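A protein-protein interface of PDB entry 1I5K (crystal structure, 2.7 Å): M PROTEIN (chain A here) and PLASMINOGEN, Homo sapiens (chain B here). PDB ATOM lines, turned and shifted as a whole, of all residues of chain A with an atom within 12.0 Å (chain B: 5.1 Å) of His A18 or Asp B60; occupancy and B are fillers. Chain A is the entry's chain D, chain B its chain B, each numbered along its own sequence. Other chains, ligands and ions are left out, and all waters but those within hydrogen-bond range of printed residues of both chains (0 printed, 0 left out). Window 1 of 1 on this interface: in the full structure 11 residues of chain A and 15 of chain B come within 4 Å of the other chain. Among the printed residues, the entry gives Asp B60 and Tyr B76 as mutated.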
ATOM      1  N   ALA A   6     -43.443  27.226 -26.388  1.00  0.00           N
ATOM      2  CA  ALA A   6     -42.318  28.034 -25.959  1.00  0.00           C
ATOM      3  C   ALA A   6     -41.188  27.209 -25.440  1.00  0.00           C
ATOM      4  O   ALA A   6     -40.054  27.621 -25.509  1.00  0.00           O
ATOM      5  CB  ALA A   6     -42.746  29.046 -24.909  1.00  0.00           C
ATOM      6  N   ASP A   7     -41.461  26.034 -24.915  1.00  0.00           N
ATOM      7  CA  ASP A   7     -40.344  25.282 -24.403  1.00  0.00           C
ATOM      8  C   ASP A   7     -39.485  24.777 -25.547  1.00  0.00           C
ATOM      9  O   ASP A   7     -38.282  24.618 -25.390  1.00  0.00           O
ATOM     10  CB  ASP A   7     -40.847  24.150 -23.530  1.00  0.00           C
ATOM     11  CG  ASP A   7     -40.717  24.472 -22.067  1.00  0.00           C
ATOM     12  OD1 ASP A   7     -41.338  23.770 -21.213  1.00  0.00           O
ATOM     13  OD2 ASP A   7     -39.975  25.436 -21.773  1.00  0.00           O
ATOM     14  N   GLU A   9     -39.154  26.360 -28.542  1.00  0.00           N
ATOM     15  CA  GLU A   9     -38.424  27.390 -29.185  1.00  0.00           C
ATOM     16  C   GLU A   9     -37.154  27.657 -28.432  1.00  0.00           C
ATOM     17  O   GLU A   9     -36.130  27.851 -29.061  1.00  0.00           O
ATOM     18  CB  GLU A   9     -39.275  28.667 -29.306  1.00  0.00           C
ATOM     19  CG  GLU A   9     -39.133  29.419 -30.687  1.00  0.00           C
ATOM     20  CD  GLU A   9     -39.412  30.965 -30.553  1.00  0.00           C
ATOM     21  OE1 GLU A   9     -40.427  31.316 -29.865  1.00  0.00           O
ATOM     22  OE2 GLU A   9     -38.638  31.818 -31.111  1.00  0.00           O
ATOM     23  N   LEU A  10     -37.204  27.657 -27.098  1.00  0.00           N
ATOM     24  CA  LEU A  10     -36.001  27.972 -26.290  1.00  0.00           C
ATOM     25  C   LEU A  10     -35.011  26.888 -26.437  1.00  0.00           C
ATOM     26  O   LEU A  10     -33.816  27.114 -26.408  1.00  0.00           O
ATOM     27  CB  LEU A  10     -36.270  28.115 -24.816  1.00  0.00           C
ATOM     28  CG  LEU A  10     -37.203  29.259 -24.511  1.00  0.00           C
ATOM     29  CD1 LEU A  10     -38.104  28.741 -23.391  1.00  0.00           C
ATOM     30  CD2 LEU A  10     -36.457  30.564 -24.146  1.00  0.00           C
ATOM     31  N   GLN A  11     -35.486  25.688 -26.609  1.00  0.00           N
ATOM     32  CA  GLN A  11     -34.512  24.660 -26.790  1.00  0.00           C
ATOM     33  C   GLN A  11     -33.689  24.831 -28.112  1.00  0.00           C
ATOM     34  O   GLN A  11     -32.491  24.607 -28.127  1.00  0.00           O
ATOM     35  CB  GLN A  11     -35.188  23.315 -26.738  1.00  0.00           C
ATOM     36  CG  GLN A  11     -34.154  22.279 -26.894  1.00  0.00           C
ATOM     37  CD  GLN A  11     -34.698  20.931 -26.629  1.00  0.00           C
ATOM     38  OE1 GLN A  11     -33.947  20.025 -26.252  1.00  0.00           O
ATOM     39  NE2 GLN A  11     -36.025  20.767 -26.812  1.00  0.00           N
ATOM     40  N   ARG A  12     -34.354  25.245 -29.184  1.00  0.00           N
ATOM     41  CA  ARG A  12     -33.745  25.459 -30.481  1.00  0.00           C
ATOM     42  C   ARG A  12     -32.776  26.621 -30.338  1.00  0.00           C
ATOM     43  O   ARG A  12     -31.670  26.609 -30.924  1.00  0.00           O
ATOM     44  CB  ARG A  12     -34.786  25.844 -31.561  1.00  0.00           C
ATOM     45  CG  ARG A  12     -35.671  24.740 -32.138  1.00  0.00           C
ATOM     46  CD  ARG A  12     -36.475  25.263 -33.413  1.00  0.00           C
ATOM     47  NE  ARG A  12     -37.650  26.114 -33.148  1.00  0.00           N
ATOM     48  CZ  ARG A  12     -38.790  25.646 -32.619  1.00  0.00           C
ATOM     49  NH1 ARG A  12     -38.908  24.346 -32.320  1.00  0.00           N
ATOM     50  NH2 ARG A  12     -39.805  26.470 -32.332  1.00  0.00           N
ATOM     51  N   LEU A  13     -33.184  27.623 -29.569  1.00  0.00           N
ATOM     52  CA  LEU A  13     -32.354  28.797 -29.387  1.00  0.00           C
ATOM     53  C   LEU A  13     -31.094  28.416 -28.596  1.00  0.00           C
ATOM     54  O   LEU A  13     -29.969  28.762 -28.951  1.00  0.00           O
ATOM     55  CB  LEU A  13     -33.154  29.880 -28.666  1.00  0.00           C
ATOM     56  CG  LEU A  13     -34.353  30.578 -29.308  1.00  0.00           C
ATOM     57  CD1 LEU A  13     -34.936  31.550 -28.322  1.00  0.00           C
ATOM     58  CD2 LEU A  13     -33.940  31.321 -30.537  1.00  0.00           C
ATOM     59  N   LYS A  14     -31.267  27.674 -27.520  1.00  0.00           N
ATOM     60  CA  LYS A  14     -30.094  27.271 -26.761  1.00  0.00           C
ATOM     61  C   LYS A  14     -29.228  26.463 -27.712  1.00  0.00           C
ATOM     62  O   LYS A  14     -28.037  26.693 -27.798  1.00  0.00           O
ATOM     63  CB  LYS A  14     -30.499  26.441 -25.603  1.00  0.00           C
ATOM     64  CG  LYS A  14     -29.371  25.972 -24.837  1.00  0.00           C
ATOM     65  CD  LYS A  14     -29.825  24.878 -23.849  1.00  0.00           C
ATOM     66  CE  LYS A  14     -28.629  23.998 -23.574  1.00  0.00           C
ATOM     67  NZ  LYS A  14     -28.942  22.708 -22.802  1.00  0.00           N
ATOM     68  N   ASN A  15     -29.820  25.527 -28.449  1.00  0.00           N
ATOM     69  CA  ASN A  15     -29.039  24.736 -29.381  1.00  0.00           C
ATOM     70  C   ASN A  15     -28.316  25.662 -30.349  1.00  0.00           C
ATOM     71  O   ASN A  15     -27.183  25.375 -30.723  1.00  0.00           O
ATOM     72  CB  ASN A  15     -29.936  23.821 -30.196  1.00  0.00           C
ATOM     73  CG  ASN A  15     -30.390  22.639 -29.434  1.00  0.00           C
ATOM     74  OD1 ASN A  15     -29.725  22.261 -28.504  1.00  0.00           O
ATOM     75  ND2 ASN A  15     -31.524  22.020 -29.833  1.00  0.00           N
ATOM     76  N   GLU A  16     -28.968  26.758 -30.780  1.00  0.00           N
ATOM     77  CA  GLU A  16     -28.315  27.658 -31.738  1.00  0.00           C
ATOM     78  C   GLU A  16     -27.118  28.401 -31.170  1.00  0.00           C
ATOM     79  O   GLU A  16     -26.025  28.387 -31.751  1.00  0.00           O
ATOM     80  CB  GLU A  16     -29.273  28.668 -32.306  1.00  0.00           C
ATOM     81  CG  GLU A  16     -30.438  28.046 -33.055  1.00  0.00           C
ATOM     82  CD  GLU A  16     -31.407  29.121 -33.597  1.00  0.00           C
ATOM     83  OE1 GLU A  16     -32.679  28.939 -33.470  1.00  0.00           O
ATOM     84  OE2 GLU A  16     -30.857  30.131 -34.141  1.00  0.00           O
ATOM     85  N   ARG A  17     -27.334  29.043 -30.025  1.00  0.00           N
ATOM     86  CA  ARG A  17     -26.312  29.773 -29.360  1.00  0.00           C
ATOM     87  C   ARG A  17     -25.152  28.825 -29.205  1.00  0.00           C
ATOM     88  O   ARG A  17     -24.020  29.195 -29.411  1.00  0.00           O
ATOM     89  CB  ARG A  17     -26.845  30.220 -28.012  1.00  0.00           C
ATOM     90  CG  ARG A  17     -27.138  31.705 -27.824  1.00  0.00           C
ATOM     91  CD  ARG A  17     -28.065  31.920 -26.595  1.00  0.00           C
ATOM     92  NE  ARG A  17     -27.497  31.205 -25.465  1.00  0.00           N
ATOM     93  CZ  ARG A  17     -28.043  30.170 -24.864  1.00  0.00           C
ATOM     94  NH1 ARG A  17     -27.415  29.606 -23.882  1.00  0.00           N
ATOM     95  NH2 ARG A  17     -29.229  29.730 -25.219  1.00  0.00           N
ATOM     96  N   HIS A  18     -25.431  27.594 -28.836  1.00  0.00           N
ATOM     97  CA  HIS A  18     -24.377  26.624 -28.639  1.00  0.00           C
ATOM     98  C   HIS A  18     -23.598  26.127 -29.878  1.00  0.00           C
ATOM     99  O   HIS A  18     -22.436  25.769 -29.790  1.00  0.00           O
ATOM    100  CB  HIS A  18     -24.915  25.416 -27.867  1.00  0.00           C
ATOM    101  CG  HIS A  18     -25.080  25.658 -26.413  1.00  0.00           C
ATOM    102  ND1 HIS A  18     -24.450  24.888 -25.467  1.00  0.00           N
ATOM    103  CD2 HIS A  18     -25.760  26.609 -25.734  1.00  0.00           C
ATOM    104  CE1 HIS A  18     -24.733  25.357 -24.263  1.00  0.00           C
ATOM    105  NE2 HIS A  18     -25.526  26.402 -24.398  1.00  0.00           N
ATOM    106  N   GLU A  19     -24.223  26.085 -31.043  1.00  0.00           N
ATOM    107  CA  GLU A  19     -23.492  25.635 -32.207  1.00  0.00           C
ATOM    108  C   GLU A  19     -22.581  26.769 -32.684  1.00  0.00           C
ATOM    109  O   GLU A  19     -21.436  26.538 -33.038  1.00  0.00           O
ATOM    110  CB  GLU A  19     -24.472  25.217 -33.275  1.00  0.00           C
ATOM    111  CG  GLU A  19     -25.141  23.910 -32.949  1.00  0.00           C
ATOM    112  CD  GLU A  19     -26.207  23.499 -33.967  1.00  0.00           C
ATOM    113  OE1 GLU A  19     -26.932  22.509 -33.680  1.00  0.00           O
ATOM    114  OE2 GLU A  19     -26.310  24.167 -35.038  1.00  0.00           O
ATOM    115  N   GLU A  20     -23.065  28.001 -32.679  1.00  0.00           N
ATOM    116  CA  GLU A  20     -22.186  29.014 -33.110  1.00  0.00           C
ATOM    117  C   GLU A  20     -21.071  29.110 -32.112  1.00  0.00           C
ATOM    118  O   GLU A  20     -19.965  29.402 -32.471  1.00  0.00           O
ATOM    119  CB  GLU A  20     -22.894  30.333 -33.275  1.00  0.00           C
ATOM    120  CG  GLU A  20     -23.308  30.954 -32.000  1.00  0.00           C
ATOM    121  CD  GLU A  20     -22.386  32.092 -31.456  1.00  0.00           C
ATOM    122  OE1 GLU A  20     -22.786  32.605 -30.371  1.00  0.00           O
ATOM    123  OE2 GLU A  20     -21.324  32.452 -32.087  1.00  0.00           O
ATOM    124  N   ALA A  21     -21.307  28.819 -30.854  1.00  0.00           N
ATOM    125  CA  ALA A  21     -20.204  28.938 -29.892  1.00  0.00           C
ATOM    126  C   ALA A  21     -19.086  27.931 -30.130  1.00  0.00           C
ATOM    127  O   ALA A  21     -17.934  28.254 -29.941  1.00  0.00           O
ATOM    128  CB  ALA A  21     -20.736  28.830 -28.412  1.00  0.00           C
ATOM    129  N   GLU A  22     -19.438  26.707 -30.502  1.00  0.00           N
ATOM    130  CA  GLU A  22     -18.438  25.662 -30.797  1.00  0.00           C
ATOM    131  C   GLU A  22     -17.652  26.050 -32.087  1.00  0.00           C
ATOM    132  O   GLU A  22     -16.435  25.950 -32.131  1.00  0.00           O
ATOM    133  CB  GLU A  22     -19.138  24.275 -30.886  1.00  0.00           C
ATOM    134  CG  GLU A  22     -20.040  24.055 -29.644  1.00  0.00           C
ATOM    135  CD  GLU A  22     -21.047  22.850 -29.711  1.00  0.00           C
ATOM    136  OE1 GLU A  22     -21.448  22.386 -30.840  1.00  0.00           O
ATOM    137  OE2 GLU A  22     -21.452  22.397 -28.584  1.00  0.00           O
ATOM    138  N   LEU A  23     -18.344  26.519 -33.118  1.00  0.00           N
ATOM    139  CA  LEU A  23     -17.650  26.998 -34.305  1.00  0.00           C
ATOM    140  C   LEU A  23     -16.564  27.970 -33.858  1.00  0.00           C
ATOM    141  O   LEU A  23     -15.409  27.716 -34.060  1.00  0.00           O
ATOM    142  CB  LEU A  23     -18.576  27.766 -35.217  1.00  0.00           C
ATOM    143  CG  LEU A  23     -19.304  27.069 -36.342  1.00  0.00           C
ATOM    144  CD1 LEU A  23     -19.877  28.226 -37.172  1.00  0.00           C
ATOM    145  CD2 LEU A  23     -18.402  26.124 -37.195  1.00  0.00           C
ATOM    146  N   GLU A  24     -16.965  29.093 -33.275  1.00  0.00           N
ATOM    147  CA  GLU A  24     -16.067  30.123 -32.754  1.00  0.00           C
ATOM    148  C   GLU A  24     -14.886  29.437 -32.112  1.00  0.00           C
ATOM    149  O   GLU A  24     -13.827  29.321 -32.731  1.00  0.00           O
ATOM    150  CB  GLU A  24     -16.830  30.969 -31.714  1.00  0.00           C
ATOM    151  CG  GLU A  24     -16.169  32.257 -31.116  1.00  0.00           C
ATOM    152  CD  GLU A  24     -17.217  33.205 -30.353  1.00  0.00           C
ATOM    153  OE1 GLU A  24     -17.637  32.879 -29.182  1.00  0.00           O
ATOM    154  OE2 GLU A  24     -17.636  34.253 -30.951  1.00  0.00           O
ATOM    155  N   ARG A  25     -15.088  28.948 -30.880  1.00  0.00           N
ATOM    156  CA  ARG A  25     -14.059  28.272 -30.051  1.00  0.00           C
ATOM    157  C   ARG A  25     -13.116  27.489 -30.923  1.00  0.00           C
ATOM    158  O   ARG A  25     -11.921  27.681 -30.931  1.00  0.00           O
ATOM    159  CB  ARG A  25     -14.726  27.347 -29.036  1.00  0.00           C
ATOM    160  CG  ARG A  25     -13.912  27.097 -27.736  1.00  0.00           C
ATOM    161  CD  ARG A  25     -14.556  26.108 -26.737  1.00  0.00           C
ATOM    162  NE  ARG A  25     -16.025  26.283 -26.554  1.00  0.00           N
ATOM    163  CZ  ARG A  25     -16.664  27.407 -26.147  1.00  0.00           C
ATOM    164  NH1 ARG A  25     -15.995  28.534 -25.879  1.00  0.00           N
ATOM    165  NH2 ARG A  25     -17.986  27.387 -25.929  1.00  0.00           N
ATOM    166  N   LEU A  26     -13.683  26.616 -31.704  1.00  0.00           N
ATOM    167  CA  LEU A  26     -12.889  25.796 -32.614  1.00  0.00           C
ATOM    168  C   LEU A  26     -12.270  26.636 -33.733  1.00  0.00           C
ATOM    169  O   LEU A  26     -11.211  26.334 -34.268  1.00  0.00           O
ATOM    170  CB  LEU A  26     -13.803  24.724 -33.209  1.00  0.00           C
ATOM    171  CG  LEU A  26     -13.066  23.412 -33.485  1.00  0.00           C
ATOM    172  CD1 LEU A  26     -13.207  22.959 -34.939  1.00  0.00           C
ATOM    173  CD2 LEU A  26     -11.565  23.506 -33.208  1.00  0.00           C
ATOM    174  N   LYS A  27     -12.996  27.704 -34.112  1.00  0.00           N
ATOM    175  CA  LYS A  27     -12.499  28.573 -35.172  1.00  0.00           C
ATOM    176  C   LYS A  27     -12.929  28.079 -36.554  1.00  0.00           C
ATOM    177  O   LYS A  27     -12.930  26.890 -36.845  1.00  0.00           O
ATOM    178  CB  LYS A  27     -10.972  28.609 -35.084  1.00  0.00           C
ATOM    179  CG  LYS A  27     -10.474  29.606 -34.036  1.00  0.00           C
ATOM    180  CD  LYS A  27      -8.962  29.826 -34.117  1.00  0.00           C
ATOM    181  CE  LYS A  27      -8.422  30.633 -32.932  1.00  0.00           C
ATOM    182  NZ  LYS A  27      -6.977  30.804 -33.071  1.00  0.00           N
ATOM    183  N   SER B   9     -29.136  25.801 -11.193  1.00  0.00           N
ATOM    184  CA  SER B   9     -28.531  26.220 -12.422  1.00  0.00           C
ATOM    185  C   SER B   9     -28.991  27.586 -12.857  1.00  0.00           C
ATOM    186  O   SER B   9     -28.808  27.959 -13.998  1.00  0.00           O
ATOM    187  CB  SER B   9     -28.824  25.214 -13.501  1.00  0.00           C
ATOM    188  OG  SER B   9     -27.956  24.096 -13.352  1.00  0.00           O
ATOM    189  N   ASN B  56     -31.219  32.762 -17.258  1.00  0.00           N
ATOM    190  CA  ASN B  56     -31.046  31.375 -17.774  1.00  0.00           C
ATOM    191  C   ASN B  56     -32.436  30.891 -18.074  1.00  0.00           C
ATOM    192  O   ASN B  56     -32.911  30.023 -17.417  1.00  0.00           O
ATOM    193  CB  ASN B  56     -30.502  30.405 -16.746  1.00  0.00           C
ATOM    194  CG  ASN B  56     -30.507  28.977 -17.265  1.00  0.00           C
ATOM    195  OD1 ASN B  56     -30.059  28.020 -16.608  1.00  0.00           O
ATOM    196  ND2 ASN B  56     -31.023  28.819 -18.460  1.00  0.00           N
ATOM    197  N   ASP B  58     -33.548  29.154 -20.599  1.00  0.00           N
ATOM    198  CA  ASP B  58     -33.661  27.977 -21.449  1.00  0.00           C
ATOM    199  C   ASP B  58     -32.886  26.721 -21.090  1.00  0.00           C
ATOM    200  O   ASP B  58     -32.429  26.000 -21.998  1.00  0.00           O
ATOM    201  CB  ASP B  58     -33.269  28.390 -22.859  1.00  0.00           C
ATOM    202  CG  ASP B  58     -31.855  28.905 -22.920  1.00  0.00           C
ATOM    203  OD1 ASP B  58     -31.324  29.290 -21.869  1.00  0.00           O
ATOM    204  OD2 ASP B  58     -31.272  28.958 -24.006  1.00  0.00           O
ATOM    205  N   ARG B  59     -32.743  26.438 -19.806  1.00  0.00           N
ATOM    206  CA  ARG B  59     -32.025  25.228 -19.344  1.00  0.00           C
ATOM    207  C   ARG B  59     -30.544  25.105 -19.698  1.00  0.00           C
ATOM    208  O   ARG B  59     -30.091  24.042 -20.138  1.00  0.00           O
ATOM    209  CB  ARG B  59     -32.702  23.969 -19.849  1.00  0.00           C
ATOM    210  CG  ARG B  59     -34.171  24.058 -19.707  1.00  0.00           C
ATOM    211  CD  ARG B  59     -34.889  22.919 -20.371  1.00  0.00           C
ATOM    212  NE  ARG B  59     -36.295  22.989 -20.017  1.00  0.00           N
ATOM    213  CZ  ARG B  59     -37.092  21.942 -20.058  1.00  0.00           C
ATOM    214  NH1 ARG B  59     -36.559  20.796 -20.438  1.00  0.00           N
ATOM    215  NH2 ARG B  59     -38.384  22.034 -19.731  1.00  0.00           N
ATOM    216  N   ASP B  60     -29.791  26.172 -19.510  1.00  0.00           N
ATOM    217  CA  ASP B  60     -28.417  26.099 -19.812  1.00  0.00           C
ATOM    218  C   ASP B  60     -27.780  25.909 -18.463  1.00  0.00           C
ATOM    219  O   ASP B  60     -28.406  26.049 -17.456  1.00  0.00           O
ATOM    220  CB  ASP B  60     -27.970  27.370 -20.581  1.00  0.00           C
ATOM    221  CG  ASP B  60     -26.670  27.149 -21.391  1.00  0.00           C
ATOM    222  OD1 ASP B  60     -26.319  28.026 -22.160  1.00  0.00           O
ATOM    223  OD2 ASP B  60     -25.967  26.115 -21.260  1.00  0.00           O
ATOM    224  N   LEU B  61     -26.522  25.558 -18.453  1.00  0.00           N
ATOM    225  CA  LEU B  61     -25.805  25.313 -17.221  1.00  0.00           C
ATOM    226  C   LEU B  61     -25.846  26.391 -16.111  1.00  0.00           C
ATOM    227  O   LEU B  61     -26.071  26.063 -14.930  1.00  0.00           O
ATOM    228  CB  LEU B  61     -24.358  24.983 -17.578  1.00  0.00           C
ATOM    229  CG  LEU B  61     -24.098  23.827 -18.571  1.00  0.00           C
ATOM    230  CD1 LEU B  61     -22.617  23.862 -18.880  1.00  0.00           C
ATOM    231  CD2 LEU B  61     -24.494  22.477 -18.000  1.00  0.00           C
ATOM    232  N   ARG B  62     -25.633  27.656 -16.477  1.00  0.00           N
ATOM    233  CA  ARG B  62     -25.647  28.780 -15.528  1.00  0.00           C
ATOM    234  C   ARG B  62     -26.262  29.953 -16.266  1.00  0.00           C
ATOM    235  O   ARG B  62     -26.400  29.921 -17.458  1.00  0.00           O
ATOM    236  CB  ARG B  62     -24.213  29.198 -15.103  1.00  0.00           C
ATOM    237  CG  ARG B  62     -23.312  28.088 -14.570  1.00  0.00           C
ATOM    238  CD  ARG B  62     -24.052  27.076 -13.625  1.00  0.00           C
ATOM    239  NE  ARG B  62     -23.203  26.012 -13.015  1.00  0.00           N
ATOM    240  CZ  ARG B  62     -22.145  25.396 -13.589  1.00  0.00           C
ATOM    241  NH1 ARG B  62     -21.480  24.459 -12.931  1.00  0.00           N
ATOM    242  NH2 ARG B  62     -21.718  25.721 -14.793  1.00  0.00           N
ATOM    243  N   TRP B  64     -26.722  33.212 -18.411  1.00  0.00           N
ATOM    244  CA  TRP B  64     -25.870  33.817 -19.444  1.00  0.00           C
ATOM    245  C   TRP B  64     -26.521  35.100 -19.980  1.00  0.00           C
ATOM    246  O   TRP B  64     -27.514  35.597 -19.435  1.00  0.00           O
ATOM    247  CB  TRP B  64     -25.726  32.829 -20.607  1.00  0.00           C
ATOM    248  CG  TRP B  64     -27.098  32.411 -21.095  1.00  0.00           C
ATOM    249  CD1 TRP B  64     -27.931  31.520 -20.502  1.00  0.00           C
ATOM    250  CD2 TRP B  64     -27.817  32.928 -22.239  1.00  0.00           C
ATOM    251  NE1 TRP B  64     -29.122  31.434 -21.203  1.00  0.00           N
ATOM    252  CE2 TRP B  64     -29.076  32.283 -22.266  1.00  0.00           C
ATOM    253  CE3 TRP B  64     -27.511  33.866 -23.241  1.00  0.00           C
ATOM    254  CZ2 TRP B  64     -30.028  32.548 -23.236  1.00  0.00           C
ATOM    255  CZ3 TRP B  64     -28.454  34.120 -24.206  1.00  0.00           C
ATOM    256  CH2 TRP B  64     -29.704  33.459 -24.199  1.00  0.00           C
ATOM    257  N   TRP B  74     -22.686  35.863 -26.935  1.00  0.00           N
ATOM    258  CA  TRP B  74     -23.218  35.580 -25.598  1.00  0.00           C
ATOM    259  C   TRP B  74     -22.162  34.974 -24.665  1.00  0.00           C
ATOM    260  O   TRP B  74     -21.089  34.518 -25.133  1.00  0.00           O
ATOM    261  CB  TRP B  74     -24.400  34.594 -25.657  1.00  0.00           C
ATOM    262  CG  TRP B  74     -24.054  33.221 -26.104  1.00  0.00           C
ATOM    263  CD1 TRP B  74     -23.975  32.779 -27.386  1.00  0.00           C
ATOM    264  CD2 TRP B  74     -23.803  32.077 -25.276  1.00  0.00           C
ATOM    265  NE1 TRP B  74     -23.698  31.429 -27.425  1.00  0.00           N
ATOM    266  CE2 TRP B  74     -23.588  30.977 -26.134  1.00  0.00           C
ATOM    267  CE3 TRP B  74     -23.752  31.867 -23.895  1.00  0.00           C
ATOM    268  CZ2 TRP B  74     -23.316  29.694 -25.637  1.00  0.00           C
ATOM    269  CZ3 TRP B  74     -23.491  30.611 -23.426  1.00  0.00           C
ATOM    270  CH2 TRP B  74     -23.273  29.546 -24.283  1.00  0.00           C
ATOM    271  N   TYR B  76     -21.516  33.001 -20.450  1.00  0.00           N
ATOM    272  CA  TYR B  76     -21.972  32.610 -19.126  1.00  0.00           C
ATOM    273  C   TYR B  76     -21.621  33.673 -18.131  1.00  0.00           C
ATOM    274  O   TYR B  76     -20.593  34.286 -18.208  1.00  0.00           O
ATOM    275  CB  TYR B  76     -21.357  31.233 -18.691  1.00  0.00           C
ATOM    276  CG  TYR B  76     -21.975  30.006 -19.382  1.00  0.00           C
ATOM    277  CD1 TYR B  76     -23.386  29.799 -19.381  1.00  0.00           C
ATOM    278  CD2 TYR B  76     -21.165  29.092 -20.074  1.00  0.00           C
ATOM    279  CE1 TYR B  76     -23.961  28.731 -20.069  1.00  0.00           C
ATOM    280  CE2 TYR B  76     -21.732  27.984 -20.779  1.00  0.00           C
ATOM    281  CZ  TYR B  76     -23.123  27.820 -20.777  1.00  0.00           C
ATOM    282  OH  TYR B  76     -23.680  26.791 -21.480  1.00  0.00           O
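The side-chain carboxylate (OD2) of Asp B58 is in salt-bridge range of the guanidinium group (NH2) of Arg A17 (2.5 Å). The side-chain carboxylate (OD1) of Asp A7 is in salt-bridge range of the guanidinium group (NH2) of Arg B59 (3.7 Å). NZ of Lys A14 sits at hydrogen-bond distance from O of Arg B59 (3.2 Å). The guanidinium group of Arg A17 lies within salt-bridge range of the side-chain carboxylate of Asp B60 (2.6 Å). OD1 of Asp B60 is in hydrogen-bond range of NE2 of His A18, 2.9 Å away. NE1 of Trp B74 sits at hydrogen-bond distance from O of Arg A17 (3.0 Å). The indole nitrogen of Trp B74 lies close to the side-chain carboxylate of Glu A20, 3.3 Å away. OH of Tyr B76 lies close to NE2 of His A18 (3.5 Å).
The side-chain amide nitrogen (ND2) of Asn B56 sits close to the backbone NH (N) of Asp B58, at 3.3 Å. The backbone NH (N) of Arg B59 sits close to the side-chain amide nitrogen (ND2) of Asn B56. OD1 of Asn B56 lies close to O of Asp B60 (2.7 Å). The side-chain carboxylate (OD1) of Asp B58 is in hydrogen-bond range of the indole nitrogen (NE1) of Trp B64 (3.1 Å). The side-chain carboxylate (OD1) of Asp B60 sits at hydrogen-bond distance from the side-chain hydroxyl (OH) of Tyr B76.
Among the printed residues, merely in contact across the chains: Lys A14 with Asp B58, Arg A17 with Trp B64, Leu A10 with Asp B58, His A18 with Trp B74 and Ala A21 with Trp B74.
Of the printed residues of chain B, Leu A10 touches Asp B58. Printed residues of chain B within 4 Å of Arg A17: Asp B58 (2.5 Å), Asp B60 (2.6 Å), Trp B64 (3.3 Å) and Trp B74 (3.0 Å). His A18 touches just these residues of chain B: Asp B60 (2.9 Å), Trp B74 (3.9 Å) and Tyr B76 (3.3 Å). Of the printed residues of chain B, Glu A20 touches Trp B74. Of chain A, only Leu A10 (3.6 Å), Lys A14 (3.1 Å) and Arg A17 (2.5 Å) come within 4 Å of Asp B58. Printed residues of chain A within 4 Å of Asp B60: Arg A17 (2.6 Å) and His A18 (2.9 Å). Of the printed residues of chain A, Trp B74 touches Arg A17 (3.0 Å), His A18 (3.9 Å), Glu A20 (3.2 Å) and Ala A21 (3.9 Å). Printed residues of chain A within 4 Å of Tyr B76: His A18. The nearest printed residue of chain B that does not touch Arg A17 is Tyr B76 (5.2 Å).
Of the 21 printed residues of chain A, 7 touch a printed residue of chain B. Hydrophobic or aromatic side chains of chain A that line the printed part of chain B: Leu A10, His A18 and Ala A21. Of the 10 printed residues of chain B, 6 touch a printed residue of chain A.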
